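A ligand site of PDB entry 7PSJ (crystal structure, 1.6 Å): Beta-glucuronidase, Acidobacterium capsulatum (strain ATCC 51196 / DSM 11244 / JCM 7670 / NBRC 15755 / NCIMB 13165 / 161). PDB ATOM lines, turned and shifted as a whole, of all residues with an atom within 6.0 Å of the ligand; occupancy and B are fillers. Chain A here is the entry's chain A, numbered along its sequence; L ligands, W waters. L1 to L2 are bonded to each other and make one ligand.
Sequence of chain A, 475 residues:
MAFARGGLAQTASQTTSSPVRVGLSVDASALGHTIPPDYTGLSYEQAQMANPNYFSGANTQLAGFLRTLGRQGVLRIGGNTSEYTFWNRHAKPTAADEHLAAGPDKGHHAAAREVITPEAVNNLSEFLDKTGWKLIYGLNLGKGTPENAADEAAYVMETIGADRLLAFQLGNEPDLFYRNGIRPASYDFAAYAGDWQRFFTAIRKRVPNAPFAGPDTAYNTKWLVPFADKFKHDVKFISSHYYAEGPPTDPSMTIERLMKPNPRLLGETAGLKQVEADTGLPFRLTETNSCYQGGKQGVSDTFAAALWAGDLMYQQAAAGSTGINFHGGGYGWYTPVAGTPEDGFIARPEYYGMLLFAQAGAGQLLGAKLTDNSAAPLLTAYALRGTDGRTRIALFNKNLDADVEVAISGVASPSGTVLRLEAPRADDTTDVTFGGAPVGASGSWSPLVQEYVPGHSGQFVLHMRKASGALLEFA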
ATOM      1  N   GLU A  45     -24.387 -24.320  11.511  1.00  0.00           N
ATOM      2  CA  GLU A  45     -23.519 -24.511  12.677  1.00  0.00           C
ATOM      3  C   GLU A  45     -23.858 -25.822  13.405  1.00  0.00           C
ATOM      4  O   GLU A  45     -25.019 -26.053  13.683  1.00  0.00           O
ATOM      5  CB  GLU A  45     -23.661 -23.311  13.586  1.00  0.00           C
ATOM      6  CG  GLU A  45     -23.046 -22.060  12.997  1.00  0.00           C
ATOM      7  CD  GLU A  45     -21.552 -22.060  12.730  1.00  0.00           C
ATOM      8  OE1 GLU A  45     -20.769 -22.845  13.398  1.00  0.00           O
ATOM      9  OE2 GLU A  45     -21.158 -21.305  11.798  1.00  0.00           O
ATOM     10  N   ARG A  76     -25.228 -29.692   5.253  1.00  0.00           N
ATOM     11  CA  ARG A  76     -23.901 -29.741   5.873  1.00  0.00           C
ATOM     12  C   ARG A  76     -23.988 -29.079   7.243  1.00  0.00           C
ATOM     13  O   ARG A  76     -24.440 -27.919   7.366  1.00  0.00           O
ATOM     14  CB  ARG A  76     -22.813 -29.080   5.029  1.00  0.00           C
ATOM     15  CG  ARG A  76     -21.434 -29.067   5.654  1.00  0.00           C
ATOM     16  CD  ARG A  76     -21.085 -27.769   6.315  1.00  0.00           C
ATOM     17  NE  ARG A  76     -19.751 -27.747   6.903  1.00  0.00           N
ATOM     18  CZ  ARG A  76     -19.118 -26.621   7.229  1.00  0.00           C
ATOM     19  NH1 ARG A  76     -19.694 -25.457   6.996  1.00  0.00           N
ATOM     20  NH2 ARG A  76     -17.907 -26.686   7.779  1.00  0.00           N
ATOM     21  N   GLY A  78     -21.519 -28.112  10.475  1.00  0.00           N
ATOM     22  CA  GLY A  78     -20.116 -27.960  10.825  1.00  0.00           C
ATOM     23  C   GLY A  78     -19.837 -26.583  11.358  1.00  0.00           C
ATOM     24  O   GLY A  78     -20.433 -26.203  12.387  1.00  0.00           O
ATOM     25  N   GLY A  79     -18.959 -25.858  10.685  1.00  0.00           N
ATOM     26  CA  GLY A  79     -18.727 -24.457  11.009  1.00  0.00           C
ATOM     27  C   GLY A  79     -17.840 -24.280  12.212  1.00  0.00           C
ATOM     28  O   GLY A  79     -17.318 -25.298  12.776  1.00  0.00           O
ATOM     29  N   ASN A  80     -17.560 -23.029  12.528  1.00  0.00           N
ATOM     30  CA  ASN A  80     -16.637 -22.669  13.627  1.00  0.00           C
ATOM     31  C   ASN A  80     -17.141 -23.267  14.939  1.00  0.00           C
ATOM     32  O   ASN A  80     -16.293 -23.538  15.831  1.00  0.00           O
ATOM     33  CB  ASN A  80     -16.507 -21.159  13.813  1.00  0.00           C
ATOM     34  CG  ASN A  80     -15.781 -20.500  12.670  1.00  0.00           C
ATOM     35  OD1 ASN A  80     -15.166 -21.156  11.818  1.00  0.00           O
ATOM     36  ND2 ASN A  80     -15.821 -19.171  12.657  1.00  0.00           N
ATOM     37  N   THR A  81     -18.444 -23.468  15.111  1.00  0.00           N
ATOM     38  CA  THR A  81     -18.974 -24.020  16.387  1.00  0.00           C
ATOM     39  C   THR A  81     -18.622 -25.506  16.528  1.00  0.00           C
ATOM     40  O   THR A  81     -18.689 -25.980  17.688  1.00  0.00           O
ATOM     41  CB  THR A  81     -20.481 -23.830  16.587  1.00  0.00           C
ATOM     42  OG1 THR A  81     -21.145 -24.524  15.525  1.00  0.00           O
ATOM     43  CG2 THR A  81     -20.906 -22.390  16.625  1.00  0.00           C
ATOM     44  N   ASN A 172     -13.349 -27.844  10.778  1.00  0.00           N
ATOM     45  CA  ASN A 172     -13.820 -26.797   9.842  1.00  0.00           C
ATOM     46  C   ASN A 172     -12.702 -25.773   9.703  1.00  0.00           C
ATOM     47  O   ASN A 172     -12.177 -25.374  10.749  1.00  0.00           O
ATOM     48  CB  ASN A 172     -15.065 -26.156  10.422  1.00  0.00           C
ATOM     49  CG  ASN A 172     -15.404 -24.833   9.779  1.00  0.00           C
ATOM     50  OD1 ASN A 172     -15.981 -24.836   8.690  1.00  0.00           O
ATOM     51  ND2 ASN A 172     -15.071 -23.732  10.476  1.00  0.00           N
ATOM     52  N   GLU A 173     -12.331 -25.405   8.478  1.00  0.00           N
ATOM     53  CA  GLU A 173     -11.284 -24.348   8.238  1.00  0.00           C
ATOM     54  C   GLU A 173     -10.102 -24.510   9.191  1.00  0.00           C
ATOM     55  O   GLU A 173      -9.717 -23.574   9.928  1.00  0.00           O
ATOM     56  CB  GLU A 173     -11.951 -22.972   8.307  1.00  0.00           C
ATOM     57  CG  GLU A 173     -13.089 -22.852   7.307  1.00  0.00           C
ATOM     58  CD  GLU A 173     -13.618 -21.455   7.004  1.00  0.00           C
ATOM     59  OE1 GLU A 173     -13.435 -20.594   7.838  1.00  0.00           O
ATOM     60  OE2 GLU A 173     -14.238 -21.277   5.941  1.00  0.00           O
ATOM     61  N   LEU A 176      -7.447 -21.821   9.673  1.00  0.00           N
ATOM     62  CA  LEU A 176      -7.734 -20.626  10.517  1.00  0.00           C
ATOM     63  C   LEU A 176      -7.810 -20.980  12.008  1.00  0.00           C
ATOM     64  O   LEU A 176      -8.142 -20.100  12.802  1.00  0.00           O
ATOM     65  CB  LEU A 176      -9.043 -19.995  10.009  1.00  0.00           C
ATOM     66  CG  LEU A 176      -8.997 -19.529   8.555  1.00  0.00           C
ATOM     67  CD1 LEU A 176     -10.250 -18.729   8.209  1.00  0.00           C
ATOM     68  CD2 LEU A 176      -7.756 -18.688   8.268  1.00  0.00           C
ATOM     69  N   HIS A 241     -14.497 -23.941   0.565  1.00  0.00           N
ATOM     70  CA  HIS A 241     -15.381 -22.823   0.938  1.00  0.00           C
ATOM     71  C   HIS A 241     -15.139 -21.637   0.012  1.00  0.00           C
ATOM     72  O   HIS A 241     -14.026 -21.520  -0.580  1.00  0.00           O
ATOM     73  CB  HIS A 241     -15.134 -22.426   2.402  1.00  0.00           C
ATOM     74  CG  HIS A 241     -15.374 -23.522   3.397  1.00  0.00           C
ATOM     75  ND1 HIS A 241     -15.178 -23.335   4.738  1.00  0.00           N
ATOM     76  CD2 HIS A 241     -15.905 -24.742   3.255  1.00  0.00           C
ATOM     77  CE1 HIS A 241     -15.526 -24.442   5.382  1.00  0.00           C
ATOM     78  NE2 HIS A 241     -15.980 -25.310   4.503  1.00  0.00           N
ATOM     79  N   TYR A 243     -16.234 -17.257  -0.046  1.00  0.00           N
ATOM     80  CA  TYR A 243     -16.927 -15.992   0.304  1.00  0.00           C
ATOM     81  C   TYR A 243     -16.557 -14.957  -0.750  1.00  0.00           C
ATOM     82  O   TYR A 243     -15.341 -14.772  -0.983  1.00  0.00           O
ATOM     83  CB  TYR A 243     -16.588 -15.603   1.748  1.00  0.00           C
ATOM     84  CG  TYR A 243     -16.552 -16.802   2.660  1.00  0.00           C
ATOM     85  CD1 TYR A 243     -17.730 -17.412   3.055  1.00  0.00           C
ATOM     86  CD2 TYR A 243     -15.359 -17.424   2.991  1.00  0.00           C
ATOM     87  CE1 TYR A 243     -17.706 -18.546   3.852  1.00  0.00           C
ATOM     88  CE2 TYR A 243     -15.313 -18.560   3.775  1.00  0.00           C
ATOM     89  CZ  TYR A 243     -16.500 -19.139   4.190  1.00  0.00           C
ATOM     90  OH  TYR A 243     -16.436 -20.279   4.919  1.00  0.00           O
ATOM     91  N   GLU A 287     -19.252 -24.638   2.235  1.00  0.00           N
ATOM     92  CA  GLU A 287     -19.659 -23.422   2.980  1.00  0.00           C
ATOM     93  C   GLU A 287     -19.445 -22.220   2.092  1.00  0.00           C
ATOM     94  O   GLU A 287     -18.301 -21.977   1.652  1.00  0.00           O
ATOM     95  CB  GLU A 287     -18.826 -23.324   4.257  1.00  0.00           C
ATOM     96  CG  GLU A 287     -19.357 -22.226   5.163  1.00  0.00           C
ATOM     97  CD  GLU A 287     -18.445 -22.024   6.341  1.00  0.00           C
ATOM     98  OE1 GLU A 287     -17.733 -22.944   6.753  1.00  0.00           O
ATOM     99  OE2 GLU A 287     -18.474 -20.772   6.890  1.00  0.00           O
ATOM    100  N   CYS A 291     -20.679 -12.677   2.027  1.00  0.00           N
ATOM    101  CA  CYS A 291     -19.701 -12.019   2.918  1.00  0.00           C
ATOM    102  C   CYS A 291     -19.489 -12.976   4.100  1.00  0.00           C
ATOM    103  O   CYS A 291     -20.431 -13.725   4.425  1.00  0.00           O
ATOM    104  CB  CYS A 291     -20.193 -10.642   3.361  1.00  0.00           C
ATOM    105  SG  CYS A 291     -20.421  -9.417   2.031  1.00  0.00           S
ATOM    106  N   TYR A 292     -18.272 -13.031   4.643  1.00  0.00           N
ATOM    107  CA  TYR A 292     -17.939 -13.805   5.861  1.00  0.00           C
ATOM    108  C   TYR A 292     -18.170 -12.895   7.065  1.00  0.00           C
ATOM    109  O   TYR A 292     -18.742 -11.807   6.913  1.00  0.00           O
ATOM    110  CB  TYR A 292     -16.552 -14.440   5.754  1.00  0.00           C
ATOM    111  CG  TYR A 292     -15.409 -13.483   5.572  1.00  0.00           C
ATOM    112  CD1 TYR A 292     -14.853 -12.838   6.669  1.00  0.00           C
ATOM    113  CD2 TYR A 292     -14.801 -13.308   4.333  1.00  0.00           C
ATOM    114  CE1 TYR A 292     -13.778 -11.979   6.524  1.00  0.00           C
ATOM    115  CE2 TYR A 292     -13.726 -12.457   4.166  1.00  0.00           C
ATOM    116  CZ  TYR A 292     -13.207 -11.795   5.271  1.00  0.00           C
ATOM    117  OH  TYR A 292     -12.152 -10.934   5.139  1.00  0.00           O
ATOM    118  N   GLN A 293     -17.868 -13.418   8.256  1.00  0.00           N
ATOM    119  CA  GLN A 293     -18.223 -12.814   9.555  1.00  0.00           C
ATOM    120  C   GLN A 293     -19.711 -12.522   9.596  1.00  0.00           C
ATOM    121  O   GLN A 293     -20.115 -11.510  10.163  1.00  0.00           O
ATOM    122  CB  GLN A 293     -17.354 -11.582   9.811  1.00  0.00           C
ATOM    123  CG  GLN A 293     -16.061 -11.911  10.538  1.00  0.00           C
ATOM    124  CD  GLN A 293     -15.144 -10.712  10.529  1.00  0.00           C
ATOM    125  OE1 GLN A 293     -15.553  -9.603  10.875  1.00  0.00           O
ATOM    126  NE2 GLN A 293     -13.918 -10.918  10.072  1.00  0.00           N
ATOM    127  N   GLY A 294     -20.526 -13.436   9.118  1.00  0.00           N
ATOM    128  CA  GLY A 294     -21.975 -13.419   9.314  1.00  0.00           C
ATOM    129  C   GLY A 294     -22.731 -12.582   8.272  1.00  0.00           C
ATOM    130  O   GLY A 294     -23.949 -12.504   8.376  1.00  0.00           O
ATOM    131  N   GLY A 295     -22.044 -12.056   7.260  1.00  0.00           N
ATOM    132  CA  GLY A 295     -22.670 -11.259   6.186  1.00  0.00           C
ATOM    133  C   GLY A 295     -22.595  -9.782   6.492  1.00  0.00           C
ATOM    134  O   GLY A 295     -22.254  -9.409   7.648  1.00  0.00           O
ATOM    135  N   HIS A 327     -24.214 -20.946   3.742  1.00  0.00           N
ATOM    136  CA  HIS A 327     -24.140 -20.912   5.214  1.00  0.00           C
ATOM    137  C   HIS A 327     -25.217 -20.001   5.800  1.00  0.00           C
ATOM    138  O   HIS A 327     -25.577 -18.983   5.203  1.00  0.00           O
ATOM    139  CB  HIS A 327     -22.762 -20.478   5.725  1.00  0.00           C
ATOM    140  CG  HIS A 327     -22.520 -20.942   7.117  1.00  0.00           C
ATOM    141  ND1 HIS A 327     -22.419 -22.295   7.464  1.00  0.00           N
ATOM    142  CD2 HIS A 327     -22.329 -20.244   8.268  1.00  0.00           C
ATOM    143  CE1 HIS A 327     -22.200 -22.400   8.747  1.00  0.00           C
ATOM    144  NE2 HIS A 327     -22.100 -21.173   9.268  1.00  0.00           N
ATOM    145  N   GLY A 328     -25.760 -20.402   6.944  1.00  0.00           N
ATOM    146  CA  GLY A 328     -26.857 -19.642   7.560  1.00  0.00           C
ATOM    147  C   GLY A 328     -27.262 -20.223   8.890  1.00  0.00           C
ATOM    148  O   GLY A 328     -26.517 -21.041   9.436  1.00  0.00           O
ATOM    149  N   GLY A 329     -28.415 -19.789   9.369  1.00  0.00           N
ATOM    150  CA  GLY A 329     -28.938 -20.055  10.731  1.00  0.00           C
ATOM    151  C   GLY A 329     -29.247 -18.757  11.451  1.00  0.00           C
ATOM    152  O   GLY A 329     -28.650 -17.648  11.125  1.00  0.00           O
ATOM    153  N   GLY A 330     -30.168 -18.852  12.381  1.00  0.00           N
ATOM    154  CA  GLY A 330     -30.559 -17.695  13.200  1.00  0.00           C
ATOM    155  C   GLY A 330     -31.233 -16.646  12.332  1.00  0.00           C
ATOM    156  O   GLY A 330     -32.033 -17.000  11.435  1.00  0.00           O
ATOM    157  N   TYR A 334     -26.766 -13.107   6.118  1.00  0.00           N
ATOM    158  CA  TYR A 334     -26.613 -13.885   4.876  1.00  0.00           C
ATOM    159  C   TYR A 334     -27.506 -15.115   4.873  1.00  0.00           C
ATOM    160  O   TYR A 334     -27.495 -15.782   3.863  1.00  0.00           O
ATOM    161  CB  TYR A 334     -25.161 -14.242   4.555  1.00  0.00           C
ATOM    162  CG  TYR A 334     -24.370 -15.002   5.597  1.00  0.00           C
ATOM    163  CD1 TYR A 334     -24.968 -15.858   6.523  1.00  0.00           C
ATOM    164  CD2 TYR A 334     -22.993 -14.875   5.638  1.00  0.00           C
ATOM    165  CE1 TYR A 334     -24.196 -16.534   7.456  1.00  0.00           C
ATOM    166  CE2 TYR A 334     -22.216 -15.527   6.567  1.00  0.00           C
ATOM    167  CZ  TYR A 334     -22.824 -16.351   7.504  1.00  0.00           C
ATOM    168  OH  TYR A 334     -22.062 -17.001   8.424  1.00  0.00           O
HETATM  169  C1  LIG L   1     -18.671 -20.237   9.895  1.00  0.00           C
HETATM  170  C2  LIG L   1     -18.572 -18.201   8.441  1.00  0.00           C
HETATM  171  C3  LIG L   1     -18.536 -16.738   8.494  1.00  0.00           C
HETATM  172  O1  LIG L   1     -18.806 -20.822  11.205  1.00  0.00           O
HETATM  173  O2  LIG L   1     -19.897 -18.211  10.463  1.00  0.00           O
HETATM  174  C4  LIG L   1     -17.533 -20.236   7.810  1.00  0.00           C
HETATM  175  C5  LIG L   1     -17.427 -20.769   9.202  1.00  0.00           C
HETATM  176  C6  LIG L   1     -18.665 -18.695   9.901  1.00  0.00           C
HETATM  177  C7  LIG L   1     -17.368 -18.803   7.677  1.00  0.00           C
HETATM  178  O3  LIG L   1     -17.438 -22.193   9.295  1.00  0.00           O
HETATM  179  O4  LIG L   1     -19.641 -16.087   8.281  1.00  0.00           O
HETATM  180  O5  LIG L   1     -17.476 -16.136   8.744  1.00  0.00           O
HETATM  181  O6  LIG L   1     -16.181 -18.326   8.268  1.00  0.00           O
HETATM  182  C1  LG2 L   2     -20.042 -18.146  11.876  1.00  0.00           C
HETATM  183  C2  LG2 L   2     -21.316 -17.328  12.166  1.00  0.00           C
HETATM  184  C3  LG2 L   2     -21.090 -15.869  11.869  1.00  0.00           C
HETATM  185  C4  LG2 L   2     -19.890 -15.377  12.631  1.00  0.00           C
HETATM  186  C5  LG2 L   2     -18.680 -16.215  12.151  1.00  0.00           C
HETATM  187  C6  LG2 L   2     -17.366 -15.719  12.759  1.00  0.00           C
HETATM  188  C7  LG2 L   2     -23.450 -18.505  11.884  1.00  0.00           C
HETATM  189  C8  LG2 L   2     -24.463 -18.975  10.905  1.00  0.00           C
HETATM  190  O1  LG2 L   2     -18.936 -17.530  12.526  1.00  0.00           O
HETATM  191  O2  LG2 L   2     -22.259 -15.134  12.283  1.00  0.00           O
HETATM  192  O3  LG2 L   2     -19.714 -13.994  12.324  1.00  0.00           O
HETATM  193  O4  LG2 L   2     -17.519 -15.799  14.182  1.00  0.00           O
HETATM  194  O5  LG2 L   2     -23.561 -18.693  13.092  1.00  0.00           O
HETATM  195  N1  LG2 L   2     -22.411 -17.836  11.360  1.00  0.00           N
HETATM  196  O   HOH W   1     -25.843 -20.355  13.700  1.00  0.00           O
HETATM  197  O   HOH W   2     -26.686 -16.769   9.517  1.00  0.00           O
HETATM  198  O   HOH W   3     -24.936 -15.372  11.278  1.00  0.00           O
HETATM  199  O   HOH W   4     -19.285 -18.901  15.205  1.00  0.00           O
HETATM  200  O   HOH W   5     -21.937 -19.071  15.309  1.00  0.00           O
HETATM  201  O   HOH W   6     -13.811 -18.130   6.759  1.00  0.00           O
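A carbon (C4) of LIG L1 is bonded to the side-chain carboxylate of Glu 287, at 1.4 Å.
OE2 of Glu 45 is in hydrogen-bond range of O1 of LIG L1 (2.5 Å).
An oxygen (O4) of LIG L1 sits at hydrogen-bond distance from the side-chain hydroxyl (OH) of Tyr 334, 2.6 Å away.
The backbone NH (N) of Gln 293 lies within hydrogen-bond range of an oxygen (O5) of LIG L1 (2.8 Å).
The backbone carbonyl oxygen (O) of Gln 293 sits close to an oxygen (O3) of LG2 L2 (3.3 Å).
The backbone NH (N) of Asn 80 sits at hydrogen-bond distance from an oxygen (O1) of LIG L1 (2.9 Å).
The backbone NH (N) of Gly 294 sits at hydrogen-bond distance from an oxygen (O4) of LIG L1 (2.9 Å).
ND2 of Asn 172 is in hydrogen-bond range of O3 of LIG L1 (3.1 Å).
The side-chain carboxylate of Glu 287 lies within salt-bridge range of the guanidinium group of Arg 76 (3.2 Å).
OE1 of Glu 287 lies close to ND1 of His 241 (3.3 Å).
The side-chain carboxylate (OE1) of Glu 45 sits at hydrogen-bond distance from the backbone NH (N) of Asn 80 (3.3 Å).
The side-chain carboxylate (OE2) of Glu 45 is in hydrogen-bond range of a ring nitrogen (NE2) of His 327 (2.7 Å).
OE1 of Glu 45 lies within hydrogen-bond range of OG1 of Thr 81, at 2.7 Å.
The side-chain amide oxygen (OD1) of Asn 172 lies within hydrogen-bond range of the guanidinium group (NH2) of Arg 76 (2.8 Å).
OH of Tyr 243 lies within hydrogen-bond range of OE2 of Glu 173 (2.6 Å).
The side-chain hydroxyl (OH) of Tyr 243 sits at hydrogen-bond distance from a ring nitrogen (ND1) of His 241 (3.3 Å).
Residues that only touch the ligand: Gly 79, Glu 173, Tyr 243, Tyr 292, His 327 and Gly 328.
Hydrophobic or aromatic side chains that line the ligand: Tyr 243, Tyr 292, His 327 and Tyr 334.
Within 4 Å of the ligand: Glu 45, Gly 79, Asn 80, Asn 172, Glu 173, Tyr 243, Glu 287, Tyr 292, Gln 293, Gly 294, His 327, Gly 328 and Tyr 334.
Along chain A the residues within 4 Å of the ligand span positions 45 to 334.
Water W6 lies within hydrogen-bond range of OE1 of Glu 173 and O6 of LIG L1.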
